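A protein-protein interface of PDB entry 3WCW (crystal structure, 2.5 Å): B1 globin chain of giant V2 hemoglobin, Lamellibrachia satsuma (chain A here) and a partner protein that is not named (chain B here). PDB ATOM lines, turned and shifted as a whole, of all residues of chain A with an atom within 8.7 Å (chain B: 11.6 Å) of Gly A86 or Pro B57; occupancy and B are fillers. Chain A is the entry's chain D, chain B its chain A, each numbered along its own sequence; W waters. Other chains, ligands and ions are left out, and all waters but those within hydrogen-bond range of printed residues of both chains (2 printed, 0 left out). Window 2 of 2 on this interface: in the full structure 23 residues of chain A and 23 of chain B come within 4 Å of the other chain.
The side-chain hydroxyl of Ser A90 is in hydrogen-bond range of the backbone carbonyl oxygen of Pro B57, 3.5 Å away. The side-chain amino group (NZ) of Lys B60 lies within salt-bridge range of the side-chain carboxylate (OD2) of Asp A84 (3.3 Å).
The side-chain carboxylate of Asp A84 is in hydrogen-bond range of the side-chain hydroxyl of Thr A87.
OH of Tyr A81 touches CB of Ala B25, at 3.9 Å. Tyr A81 touches Ala B64. CB of Pro B57 touches O of Gly A86, at 3.7 Å. Pro B57 touches Thr A87 (CB to N, 3.97 Å). Lys B60 touches Thr A87 (CE to OG1, 3.2 Å). Thr A87 touches Ala B61 (CG2 to N, 3.8 Å). CA of Gln B58 touches OG of Ser A90, at 3.8 Å. Ser A90 touches Ala B61 (OG to CB, 3.4 Å). Leu A91 touches Ala B61. CD2 of Leu A91 touches NH1 of Arg B65, 3.9 Å away.
Of the printed residues of chain B, Tyr A81 touches Ala B25 (3.9 Å) and Ala B64 (3.5 Å). Leu A82 touches none of the printed residues of chain B. Asp A84 touches one residue of chain B. No residue of chain B comes within 4 Å of Ala A85. Gly A86 touches just one residue of chain B: Pro B57 (3.7 Å). No residue of chain B comes within 4 Å of Thr A89. Thr A92 touches none of the printed residues of chain B. Of the printed residues of chain A, Ala B25 touches Tyr A81 (3.9 Å). Printed residues of chain A within 4 Å of Pro B57: Gly A86 (3.7 Å), Thr A87 (3.97 Å) and Ser A90 (3.5 Å). Printed residues of chain A within 4 Å of Lys B60: Asp A84 (3.3 Å) and Thr A87 (3.2 Å). Of the printed residues of chain A, Arg B65 touches Leu A91.
Of the 14 printed residues of chain A, 6 touch a printed residue of chain B. Hydrophobic or aromatic side chains of chain A within 4 Å of the printed part of chain B: Tyr A81 and Leu A91. Among the printed residues, 12 pairs touch across the chains. Among the printed residues, Asp or Glu carboxylates within 4 Å of a Lys or Arg side-chain nitrogen of the other chain: Asp A84 with Lys B60 (3.3 Å).
Water W1 bridges O of Leu A91 and NH1 of Arg B65. Water W2 bridges OG of Ser A90 (3.0 Å) and NH1 of Arg B65 (3.0 Å).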
ATOM      1  N   PHE A   3       0.423 -36.335   2.127  1.00  0.00           N
ATOM      2  CA  PHE A   3       1.271 -36.701   3.255  1.00  0.00           C
ATOM      3  C   PHE A   3       0.511 -37.172   4.490  1.00  0.00           C
ATOM      4  O   PHE A   3       0.504 -38.363   4.806  1.00  0.00           O
ATOM      5  CB  PHE A   3       2.177 -35.532   3.627  1.00  0.00           C
ATOM      6  CG  PHE A   3       3.244 -35.262   2.607  1.00  0.00           C
ATOM      7  CD1 PHE A   3       2.974 -34.480   1.488  1.00  0.00           C
ATOM      8  CD2 PHE A   3       4.511 -35.837   2.741  1.00  0.00           C
ATOM      9  CE1 PHE A   3       3.940 -34.275   0.519  1.00  0.00           C
ATOM     10  CE2 PHE A   3       5.485 -35.643   1.783  1.00  0.00           C
ATOM     11  CZ  PHE A   3       5.202 -34.860   0.666  1.00  0.00           C
ATOM     12  N   TYR A  81       6.044 -27.773   6.982  1.00  0.00           N
ATOM     13  CA  TYR A  81       5.398 -27.628   5.685  1.00  0.00           C
ATOM     14  C   TYR A  81       4.394 -28.748   5.396  1.00  0.00           C
ATOM     15  O   TYR A  81       3.858 -28.844   4.300  1.00  0.00           O
ATOM     16  CB  TYR A  81       6.467 -27.540   4.592  1.00  0.00           C
ATOM     17  CG  TYR A  81       6.954 -26.123   4.394  1.00  0.00           C
ATOM     18  CD1 TYR A  81       6.237 -25.230   3.595  1.00  0.00           C
ATOM     19  CD2 TYR A  81       8.065 -25.646   5.075  1.00  0.00           C
ATOM     20  CE1 TYR A  81       6.609 -23.894   3.486  1.00  0.00           C
ATOM     21  CE2 TYR A  81       8.450 -24.301   4.975  1.00  0.00           C
ATOM     22  CZ  TYR A  81       7.712 -23.433   4.178  1.00  0.00           C
ATOM     23  OH  TYR A  81       8.067 -22.104   4.076  1.00  0.00           O
ATOM     24  N   LEU A  82       4.118 -29.574   6.400  1.00  0.00           N
ATOM     25  CA  LEU A  82       3.187 -30.673   6.226  1.00  0.00           C
ATOM     26  C   LEU A  82       1.845 -30.228   5.669  1.00  0.00           C
ATOM     27  O   LEU A  82       1.267 -30.914   4.826  1.00  0.00           O
ATOM     28  CB  LEU A  82       3.004 -31.427   7.545  1.00  0.00           C
ATOM     29  CG  LEU A  82       4.151 -32.421   7.787  1.00  0.00           C
ATOM     30  CD1 LEU A  82       4.188 -32.878   9.228  1.00  0.00           C
ATOM     31  CD2 LEU A  82       3.989 -33.602   6.832  1.00  0.00           C
ATOM     32  N   ASN A  83       1.346 -29.082   6.111  1.00  0.00           N
ATOM     33  CA  ASN A  83       0.066 -28.617   5.601  1.00  0.00           C
ATOM     34  C   ASN A  83       0.177 -27.765   4.347  1.00  0.00           C
ATOM     35  O   ASN A  83      -0.687 -26.922   4.086  1.00  0.00           O
ATOM     36  CB  ASN A  83      -0.722 -27.869   6.682  1.00  0.00           C
ATOM     37  CG  ASN A  83      -1.402 -28.819   7.653  1.00  0.00           C
ATOM     38  OD1 ASN A  83      -1.860 -29.895   7.251  1.00  0.00           O
ATOM     39  ND2 ASN A  83      -1.476 -28.434   8.926  1.00  0.00           N
ATOM     40  N   ASP A  84       1.244 -27.985   3.581  1.00  0.00           N
ATOM     41  CA  ASP A  84       1.459 -27.274   2.318  1.00  0.00           C
ATOM     42  C   ASP A  84       1.984 -28.336   1.350  1.00  0.00           C
ATOM     43  O   ASP A  84       3.132 -28.285   0.905  1.00  0.00           O
ATOM     44  CB  ASP A  84       2.487 -26.145   2.479  1.00  0.00           C
ATOM     45  CG  ASP A  84       2.466 -25.154   1.304  1.00  0.00           C
ATOM     46  OD1 ASP A  84       2.156 -25.580   0.154  1.00  0.00           O
ATOM     47  OD2 ASP A  84       2.773 -23.952   1.532  1.00  0.00           O
ATOM     48  N   ALA A  85       1.119 -29.300   1.051  1.00  0.00           N
ATOM     49  CA  ALA A  85       1.433 -30.430   0.182  1.00  0.00           C
ATOM     50  C   ALA A  85       2.252 -30.071  -1.057  1.00  0.00           C
ATOM     51  O   ALA A  85       3.192 -30.786  -1.419  1.00  0.00           O
ATOM     52  CB  ALA A  85       0.143 -31.137  -0.228  1.00  0.00           C
ATOM     53  N   GLY A  86       1.896 -28.973  -1.713  1.00  0.00           N
ATOM     54  CA  GLY A  86       2.637 -28.574  -2.898  1.00  0.00           C
ATOM     55  C   GLY A  86       4.095 -28.258  -2.590  1.00  0.00           C
ATOM     56  O   GLY A  86       5.013 -28.867  -3.156  1.00  0.00           O
ATOM     57  N   THR A  87       4.310 -27.314  -1.679  1.00  0.00           N
ATOM     58  CA  THR A  87       5.660 -26.916  -1.326  1.00  0.00           C
ATOM     59  C   THR A  87       6.477 -28.059  -0.734  1.00  0.00           C
ATOM     60  O   THR A  87       7.691 -28.128  -0.938  1.00  0.00           O
ATOM     61  CB  THR A  87       5.659 -25.741  -0.336  1.00  0.00           C
ATOM     62  OG1 THR A  87       4.959 -24.632  -0.907  1.00  0.00           O
ATOM     63  CG2 THR A  87       7.075 -25.303  -0.030  1.00  0.00           C
ATOM     64  N   LEU A  88       5.822 -28.965  -0.017  1.00  0.00           N
ATOM     65  CA  LEU A  88       6.541 -30.075   0.596  1.00  0.00           C
ATOM     66  C   LEU A  88       6.988 -31.091  -0.451  1.00  0.00           C
ATOM     67  O   LEU A  88       8.067 -31.668  -0.338  1.00  0.00           O
ATOM     68  CB  LEU A  88       5.675 -30.739   1.667  1.00  0.00           C
ATOM     69  CG  LEU A  88       6.369 -31.771   2.569  1.00  0.00           C
ATOM     70  CD1 LEU A  88       7.675 -31.227   3.146  1.00  0.00           C
ATOM     71  CD2 LEU A  88       5.414 -32.145   3.678  1.00  0.00           C
ATOM     72  N   THR A  89       6.169 -31.302  -1.476  1.00  0.00           N
ATOM     73  CA  THR A  89       6.535 -32.227  -2.538  1.00  0.00           C
ATOM     74  C   THR A  89       7.832 -31.699  -3.146  1.00  0.00           C
ATOM     75  O   THR A  89       8.772 -32.460  -3.418  1.00  0.00           O
ATOM     76  CB  THR A  89       5.473 -32.272  -3.634  1.00  0.00           C
ATOM     77  OG1 THR A  89       4.211 -32.615  -3.052  1.00  0.00           O
ATOM     78  CG2 THR A  89       5.853 -33.307  -4.699  1.00  0.00           C
ATOM     79  N   SER A  90       7.870 -30.385  -3.347  1.00  0.00           N
ATOM     80  CA  SER A  90       9.042 -29.727  -3.892  1.00  0.00           C
ATOM     81  C   SER A  90      10.237 -29.830  -2.934  1.00  0.00           C
ATOM     82  O   SER A  90      11.333 -30.200  -3.340  1.00  0.00           O
ATOM     83  CB  SER A  90       8.723 -28.265  -4.157  1.00  0.00           C
ATOM     84  OG  SER A  90       9.809 -27.634  -4.802  1.00  0.00           O
ATOM     85  N   LEU A  91      10.011 -29.507  -1.663  1.00  0.00           N
ATOM     86  CA  LEU A  91      11.043 -29.560  -0.630  1.00  0.00           C
ATOM     87  C   LEU A  91      11.647 -30.953  -0.470  1.00  0.00           C
ATOM     88  O   LEU A  91      12.846 -31.105  -0.209  1.00  0.00           O
ATOM     89  CB  LEU A  91      10.454 -29.114   0.712  1.00  0.00           C
ATOM     90  CG  LEU A  91      10.244 -27.606   0.889  1.00  0.00           C
ATOM     91  CD1 LEU A  91       9.463 -27.322   2.170  1.00  0.00           C
ATOM     92  CD2 LEU A  91      11.600 -26.916   0.928  1.00  0.00           C
ATOM     93  N   THR A  92      10.804 -31.972  -0.612  1.00  0.00           N
ATOM     94  CA  THR A  92      11.245 -33.350  -0.485  1.00  0.00           C
ATOM     95  C   THR A  92      11.955 -33.842  -1.734  1.00  0.00           C
ATOM     96  O   THR A  92      12.850 -34.677  -1.635  1.00  0.00           O
ATOM     97  CB  THR A  92      10.065 -34.292  -0.181  1.00  0.00           C
ATOM     98  OG1 THR A  92       9.071 -34.187  -1.218  1.00  0.00           O
ATOM     99  CG2 THR A  92       9.463 -33.940   1.178  1.00  0.00           C
ATOM    100  N   ALA A  93      11.561 -33.345  -2.907  1.00  0.00           N
ATOM    101  CA  ALA A  93      12.226 -33.757  -4.151  1.00  0.00           C
ATOM    102  C   ALA A  93      13.671 -33.266  -4.095  1.00  0.00           C
ATOM    103  O   ALA A  93      14.598 -33.990  -4.471  1.00  0.00           O
ATOM    104  CB  ALA A  93      11.529 -33.164  -5.353  1.00  0.00           C
ATOM    105  N   ALA B  25       6.633 -18.689   6.759  1.00  0.00           N
ATOM    106  CA  ALA B  25       6.431 -18.557   5.322  1.00  0.00           C
ATOM    107  C   ALA B  25       6.103 -17.104   4.992  1.00  0.00           C
ATOM    108  O   ALA B  25       6.562 -16.585   3.981  1.00  0.00           O
ATOM    109  CB  ALA B  25       5.302 -19.474   4.849  1.00  0.00           C
ATOM    110  N   ASN B  29       8.278 -14.842   2.594  1.00  0.00           N
ATOM    111  CA  ASN B  29       7.794 -14.155   1.397  1.00  0.00           C
ATOM    112  C   ASN B  29       8.050 -12.648   1.444  1.00  0.00           C
ATOM    113  O   ASN B  29       8.258 -12.023   0.402  1.00  0.00           O
ATOM    114  CB  ASN B  29       6.298 -14.446   1.176  1.00  0.00           C
ATOM    115  CG  ASN B  29       5.687 -13.588   0.065  1.00  0.00           C
ATOM    116  OD1 ASN B  29       5.179 -12.492   0.320  1.00  0.00           O
ATOM    117  ND2 ASN B  29       5.750 -14.077  -1.173  1.00  0.00           N
ATOM    118  N   PHE B  46      17.312 -16.331 -10.256  1.00  0.00           N
ATOM    119  CA  PHE B  46      16.605 -17.442  -9.650  1.00  0.00           C
ATOM    120  C   PHE B  46      15.622 -18.190 -10.532  1.00  0.00           C
ATOM    121  O   PHE B  46      14.581 -18.645 -10.055  1.00  0.00           O
ATOM    122  CB  PHE B  46      15.892 -16.940  -8.404  1.00  0.00           C
ATOM    123  CG  PHE B  46      16.819 -16.446  -7.354  1.00  0.00           C
ATOM    124  CD1 PHE B  46      17.422 -17.338  -6.471  1.00  0.00           C
ATOM    125  CD2 PHE B  46      17.122 -15.089  -7.263  1.00  0.00           C
ATOM    126  CE1 PHE B  46      18.310 -16.887  -5.509  1.00  0.00           C
ATOM    127  CE2 PHE B  46      18.012 -14.622  -6.305  1.00  0.00           C
ATOM    128  CZ  PHE B  46      18.608 -15.519  -5.427  1.00  0.00           C
ATOM    129  N   LYS B  47      15.949 -18.326 -11.814  1.00  0.00           N
ATOM    130  CA  LYS B  47      15.079 -19.057 -12.731  1.00  0.00           C
ATOM    131  C   LYS B  47      15.044 -20.544 -12.368  1.00  0.00           C
ATOM    132  O   LYS B  47      14.070 -21.232 -12.664  1.00  0.00           O
ATOM    133  CB  LYS B  47      15.541 -18.870 -14.185  1.00  0.00           C
ATOM    134  CG  LYS B  47      15.059 -17.550 -14.799  1.00  0.00           C
ATOM    135  CD  LYS B  47      15.504 -17.375 -16.254  1.00  0.00           C
ATOM    136  CE  LYS B  47      16.972 -16.953 -16.358  1.00  0.00           C
ATOM    137  NZ  LYS B  47      17.907 -17.928 -15.711  1.00  0.00           N
ATOM    138  N   SER B  48      16.096 -21.023 -11.704  1.00  0.00           N
ATOM    139  CA  SER B  48      16.180 -22.424 -11.302  1.00  0.00           C
ATOM    140  C   SER B  48      15.219 -22.798 -10.172  1.00  0.00           C
ATOM    141  O   SER B  48      15.160 -23.955  -9.756  1.00  0.00           O
ATOM    142  CB  SER B  48      17.610 -22.766 -10.880  1.00  0.00           C
ATOM    143  OG  SER B  48      18.054 -21.915  -9.832  1.00  0.00           O
ATOM    144  N   VAL B  49      14.482 -21.816  -9.663  1.00  0.00           N
ATOM    145  CA  VAL B  49      13.520 -22.062  -8.592  1.00  0.00           C
ATOM    146  C   VAL B  49      12.257 -21.249  -8.874  1.00  0.00           C
ATOM    147  O   VAL B  49      11.576 -20.791  -7.960  1.00  0.00           O
ATOM    148  CB  VAL B  49      14.115 -21.705  -7.170  1.00  0.00           C
ATOM    149  CG1 VAL B  49      15.104 -22.781  -6.732  1.00  0.00           C
ATOM    150  CG2 VAL B  49      14.814 -20.349  -7.199  1.00  0.00           C
ATOM    151  N   LYS B  50      11.966 -21.099 -10.166  1.00  0.00           N
ATOM    152  CA  LYS B  50      10.810 -20.362 -10.688  1.00  0.00           C
ATOM    153  C   LYS B  50      10.427 -19.091  -9.935  1.00  0.00           C
ATOM    154  O   LYS B  50       9.310 -18.959  -9.442  1.00  0.00           O
ATOM    155  CB  LYS B  50       9.602 -21.293 -10.810  1.00  0.00           C
ATOM    156  CG  LYS B  50       9.831 -22.405 -11.818  1.00  0.00           C
ATOM    157  CD  LYS B  50       8.693 -23.417 -11.873  1.00  0.00           C
ATOM    158  CE  LYS B  50       7.399 -22.791 -12.382  1.00  0.00           C
ATOM    159  NZ  LYS B  50       6.344 -23.822 -12.605  1.00  0.00           N
ATOM    160  N   SER B  51      11.369 -18.152  -9.872  1.00  0.00           N
ATOM    161  CA  SER B  51      11.157 -16.873  -9.206  1.00  0.00           C
ATOM    162  C   SER B  51      10.200 -16.003 -10.023  1.00  0.00           C
ATOM    163  O   SER B  51       9.719 -14.978  -9.543  1.00  0.00           O
ATOM    164  CB  SER B  51      12.492 -16.134  -9.023  1.00  0.00           C
ATOM    165  OG  SER B  51      13.121 -15.858 -10.269  1.00  0.00           O
ATOM    166  N   GLU B  52       9.926 -16.407 -11.258  1.00  0.00           N
ATOM    167  CA  GLU B  52       9.021 -15.631 -12.095  1.00  0.00           C
ATOM    168  C   GLU B  52       7.616 -15.684 -11.499  1.00  0.00           C
ATOM    169  O   GLU B  52       6.757 -14.875 -11.832  1.00  0.00           O
ATOM    170  CB  GLU B  52       9.012 -16.168 -13.527  1.00  0.00           C
ATOM    171  CG  GLU B  52      10.218 -17.032 -13.859  1.00  0.00           C
ATOM    172  CD  GLU B  52       9.979 -18.484 -13.501  1.00  0.00           C
ATOM    173  OE1 GLU B  52      10.956 -19.264 -13.438  1.00  0.00           O
ATOM    174  OE2 GLU B  52       8.799 -18.838 -13.296  1.00  0.00           O
ATOM    175  N   ASP B  53       7.396 -16.651 -10.619  1.00  0.00           N
ATOM    176  CA  ASP B  53       6.121 -16.808  -9.936  1.00  0.00           C
ATOM    177  C   ASP B  53       6.441 -17.181  -8.500  1.00  0.00           C
ATOM    178  O   ASP B  53       6.675 -18.349  -8.190  1.00  0.00           O
ATOM    179  CB  ASP B  53       5.289 -17.895 -10.602  1.00  0.00           C
ATOM    180  CG  ASP B  53       4.042 -18.232  -9.821  1.00  0.00           C
ATOM    181  OD1 ASP B  53       3.462 -17.327  -9.191  1.00  0.00           O
ATOM    182  OD2 ASP B  53       3.635 -19.409  -9.851  1.00  0.00           O
ATOM    183  N   MET B  54       6.445 -16.175  -7.628  1.00  0.00           N
ATOM    184  CA  MET B  54       6.783 -16.384  -6.228  1.00  0.00           C
ATOM    185  C   MET B  54       5.827 -17.218  -5.403  1.00  0.00           C
ATOM    186  O   MET B  54       6.144 -17.591  -4.275  1.00  0.00           O
ATOM    187  CB  MET B  54       7.022 -15.040  -5.554  1.00  0.00           C
ATOM    188  CG  MET B  54       8.343 -14.412  -5.966  1.00  0.00           C
ATOM    189  SD  MET B  54       8.573 -12.799  -5.240  1.00  0.00           S
ATOM    190  CE  MET B  54       8.629 -13.265  -3.480  1.00  0.00           C
ATOM    191  N   ARG B  55       4.666 -17.528  -5.962  1.00  0.00           N
ATOM    192  CA  ARG B  55       3.690 -18.337  -5.246  1.00  0.00           C
ATOM    193  C   ARG B  55       3.860 -19.798  -5.635  1.00  0.00           C
ATOM    194  O   ARG B  55       3.290 -20.692  -5.005  1.00  0.00           O
ATOM    195  CB  ARG B  55       2.264 -17.866  -5.564  1.00  0.00           C
ATOM    196  CG  ARG B  55       2.007 -16.405  -5.209  1.00  0.00           C
ATOM    197  CD  ARG B  55       0.562 -16.000  -5.506  1.00  0.00           C
ATOM    198  NE  ARG B  55       0.190 -16.192  -6.912  1.00  0.00           N
ATOM    199  CZ  ARG B  55       0.688 -15.494  -7.930  1.00  0.00           C
ATOM    200  NH1 ARG B  55       0.281 -15.747  -9.168  1.00  0.00           N
ATOM    201  NH2 ARG B  55       1.586 -14.539  -7.716  1.00  0.00           N
ATOM    202  N   SER B  56       4.655 -20.034  -6.673  1.00  0.00           N
ATOM    203  CA  SER B  56       4.910 -21.391  -7.152  1.00  0.00           C
ATOM    204  C   SER B  56       5.576 -22.220  -6.056  1.00  0.00           C
ATOM    205  O   SER B  56       6.351 -21.699  -5.252  1.00  0.00           O
ATOM    206  CB  SER B  56       5.837 -21.358  -8.359  1.00  0.00           C
ATOM    207  OG  SER B  56       7.166 -21.086  -7.938  1.00  0.00           O
ATOM    208  N   PRO B  57       5.278 -23.526  -6.009  1.00  0.00           N
ATOM    209  CA  PRO B  57       5.887 -24.385  -4.985  1.00  0.00           C
ATOM    210  C   PRO B  57       7.416 -24.453  -5.110  1.00  0.00           C
ATOM    211  O   PRO B  57       8.119 -24.688  -4.121  1.00  0.00           O
ATOM    212  CB  PRO B  57       5.201 -25.738  -5.209  1.00  0.00           C
ATOM    213  CG  PRO B  57       4.832 -25.709  -6.685  1.00  0.00           C
ATOM    214  CD  PRO B  57       4.354 -24.286  -6.878  1.00  0.00           C
ATOM    215  N   GLN B  58       7.935 -24.245  -6.318  1.00  0.00           N
ATOM    216  CA  GLN B  58       9.382 -24.261  -6.531  1.00  0.00           C
ATOM    217  C   GLN B  58      10.054 -23.111  -5.789  1.00  0.00           C
ATOM    218  O   GLN B  58      11.088 -23.298  -5.141  1.00  0.00           O
ATOM    219  CB  GLN B  58       9.725 -24.129  -8.016  1.00  0.00           C
ATOM    220  CG  GLN B  58       9.483 -25.367  -8.845  1.00  0.00           C
ATOM    221  CD  GLN B  58       8.058 -25.873  -8.760  1.00  0.00           C
ATOM    222  OE1 GLN B  58       7.096 -25.120  -8.948  1.00  0.00           O
ATOM    223  NE2 GLN B  58       7.916 -27.167  -8.484  1.00  0.00           N
ATOM    224  N   PHE B  59       9.471 -21.918  -5.885  1.00  0.00           N
ATOM    225  CA  PHE B  59      10.063 -20.773  -5.217  1.00  0.00           C
ATOM    226  C   PHE B  59       9.826 -20.748  -3.716  1.00  0.00           C
ATOM    227  O   PHE B  59      10.664 -20.228  -2.966  1.00  0.00           O
ATOM    228  CB  PHE B  59       9.585 -19.463  -5.827  1.00  0.00           C
ATOM    229  CG  PHE B  59      10.402 -18.293  -5.401  1.00  0.00           C
ATOM    230  CD1 PHE B  59       9.939 -17.420  -4.434  1.00  0.00           C
ATOM    231  CD2 PHE B  59      11.679 -18.098  -5.930  1.00  0.00           C
ATOM    232  CE1 PHE B  59      10.735 -16.358  -3.988  1.00  0.00           C
ATOM    233  CE2 PHE B  59      12.487 -17.042  -5.494  1.00  0.00           C
ATOM    234  CZ  PHE B  59      12.013 -16.170  -4.520  1.00  0.00           C
ATOM    235  N   LYS B  60       8.694 -21.304  -3.279  1.00  0.00           N
ATOM    236  CA  LYS B  60       8.381 -21.358  -1.854  1.00  0.00           C
ATOM    237  C   LYS B  60       9.311 -22.350  -1.175  1.00  0.00           C
ATOM    238  O   LYS B  60       9.631 -22.206  -0.010  1.00  0.00           O
ATOM    239  CB  LYS B  60       6.916 -21.755  -1.611  1.00  0.00           C
ATOM    240  CG  LYS B  60       5.945 -20.603  -1.751  1.00  0.00           C
ATOM    241  CD  LYS B  60       4.625 -20.906  -1.074  1.00  0.00           C
ATOM    242  CE  LYS B  60       3.747 -21.816  -1.913  1.00  0.00           C
ATOM    243  NZ  LYS B  60       2.465 -22.163  -1.209  1.00  0.00           N
ATOM    244  N   ALA B  61       9.747 -23.355  -1.915  1.00  0.00           N
ATOM    245  CA  ALA B  61      10.668 -24.343  -1.377  1.00  0.00           C
ATOM    246  C   ALA B  61      12.029 -23.651  -1.180  1.00  0.00           C
ATOM    247  O   ALA B  61      12.762 -23.912  -0.216  1.00  0.00           O
ATOM    248  CB  ALA B  61      10.799 -25.503  -2.354  1.00  0.00           C
ATOM    249  N   HIS B  62      12.359 -22.766  -2.112  1.00  0.00           N
ATOM    250  CA  HIS B  62      13.608 -22.031  -2.036  1.00  0.00           C
ATOM    251  C   HIS B  62      13.555 -21.069  -0.858  1.00  0.00           C
ATOM    252  O   HIS B  62      14.524 -20.969  -0.097  1.00  0.00           O
ATOM    253  CB  HIS B  62      13.855 -21.246  -3.321  1.00  0.00           C
ATOM    254  CG  HIS B  62      15.038 -20.340  -3.245  1.00  0.00           C
ATOM    255  ND1 HIS B  62      16.334 -20.812  -3.216  1.00  0.00           N
ATOM    256  CD2 HIS B  62      15.122 -18.992  -3.136  1.00  0.00           C
ATOM    257  CE1 HIS B  62      17.166 -19.791  -3.090  1.00  0.00           C
ATOM    258  NE2 HIS B  62      16.457 -18.675  -3.039  1.00  0.00           N
ATOM    259  N   ILE B  63      12.431 -20.364  -0.718  1.00  0.00           N
ATOM    260  CA  ILE B  63      12.261 -19.415   0.378  1.00  0.00           C
ATOM    261  C   ILE B  63      12.458 -20.133   1.715  1.00  0.00           C
ATOM    262  O   ILE B  63      13.103 -19.612   2.628  1.00  0.00           O
ATOM    263  CB  ILE B  63      10.857 -18.789   0.370  1.00  0.00           C
ATOM    264  CG1 ILE B  63      10.695 -17.893  -0.859  1.00  0.00           C
ATOM    265  CG2 ILE B  63      10.626 -18.007   1.666  1.00  0.00           C
ATOM    266  CD1 ILE B  63       9.324 -17.239  -0.969  1.00  0.00           C
ATOM    267  N   ALA B  64      11.913 -21.340   1.805  1.00  0.00           N
ATOM    268  CA  ALA B  64      12.009 -22.144   3.014  1.00  0.00           C
ATOM    269  C   ALA B  64      13.441 -22.577   3.320  1.00  0.00           C
ATOM    270  O   ALA B  64      13.847 -22.588   4.488  1.00  0.00           O
ATOM    271  CB  ALA B  64      11.101 -23.385   2.898  1.00  0.00           C
ATOM    272  N   ARG B  65      14.203 -22.934   2.287  1.00  0.00           N
ATOM    273  CA  ARG B  65      15.580 -23.376   2.504  1.00  0.00           C
ATOM    274  C   ARG B  65      16.471 -22.221   2.939  1.00  0.00           C
ATOM    275  O   ARG B  65      17.325 -22.374   3.802  1.00  0.00           O
ATOM    276  CB  ARG B  65      16.147 -24.053   1.238  1.00  0.00           C
ATOM    277  CG  ARG B  65      15.645 -25.499   1.017  1.00  0.00           C
ATOM    278  CD  ARG B  65      16.390 -26.237  -0.116  1.00  0.00           C
ATOM    279  NE  ARG B  65      16.198 -25.613  -1.425  1.00  0.00           N
ATOM    280  CZ  ARG B  65      15.174 -25.850  -2.243  1.00  0.00           C
ATOM    281  NH1 ARG B  65      14.222 -26.716  -1.910  1.00  0.00           N
ATOM    282  NH2 ARG B  65      15.088 -25.198  -3.393  1.00  0.00           N
ATOM    283  N   VAL B  66      16.234 -21.052   2.355  1.00  0.00           N
ATOM    284  CA  VAL B  66      17.012 -19.871   2.677  1.00  0.00           C
ATOM    285  C   VAL B  66      16.786 -19.377   4.095  1.00  0.00           C
ATOM    286  O   VAL B  66      17.741 -19.032   4.787  1.00  0.00           O
ATOM    287  CB  VAL B  66      16.699 -18.715   1.718  1.00  0.00           C
ATOM    288  CG1 VAL B  66      17.525 -17.498   2.100  1.00  0.00           C
ATOM    289  CG2 VAL B  66      16.991 -19.135   0.272  1.00  0.00           C
HETATM  290  O   HOH W   1      14.789 -29.035   0.496  1.00  0.00           O
HETATM  291  O   HOH W   2      12.728 -27.727  -4.294  1.00  0.00           O
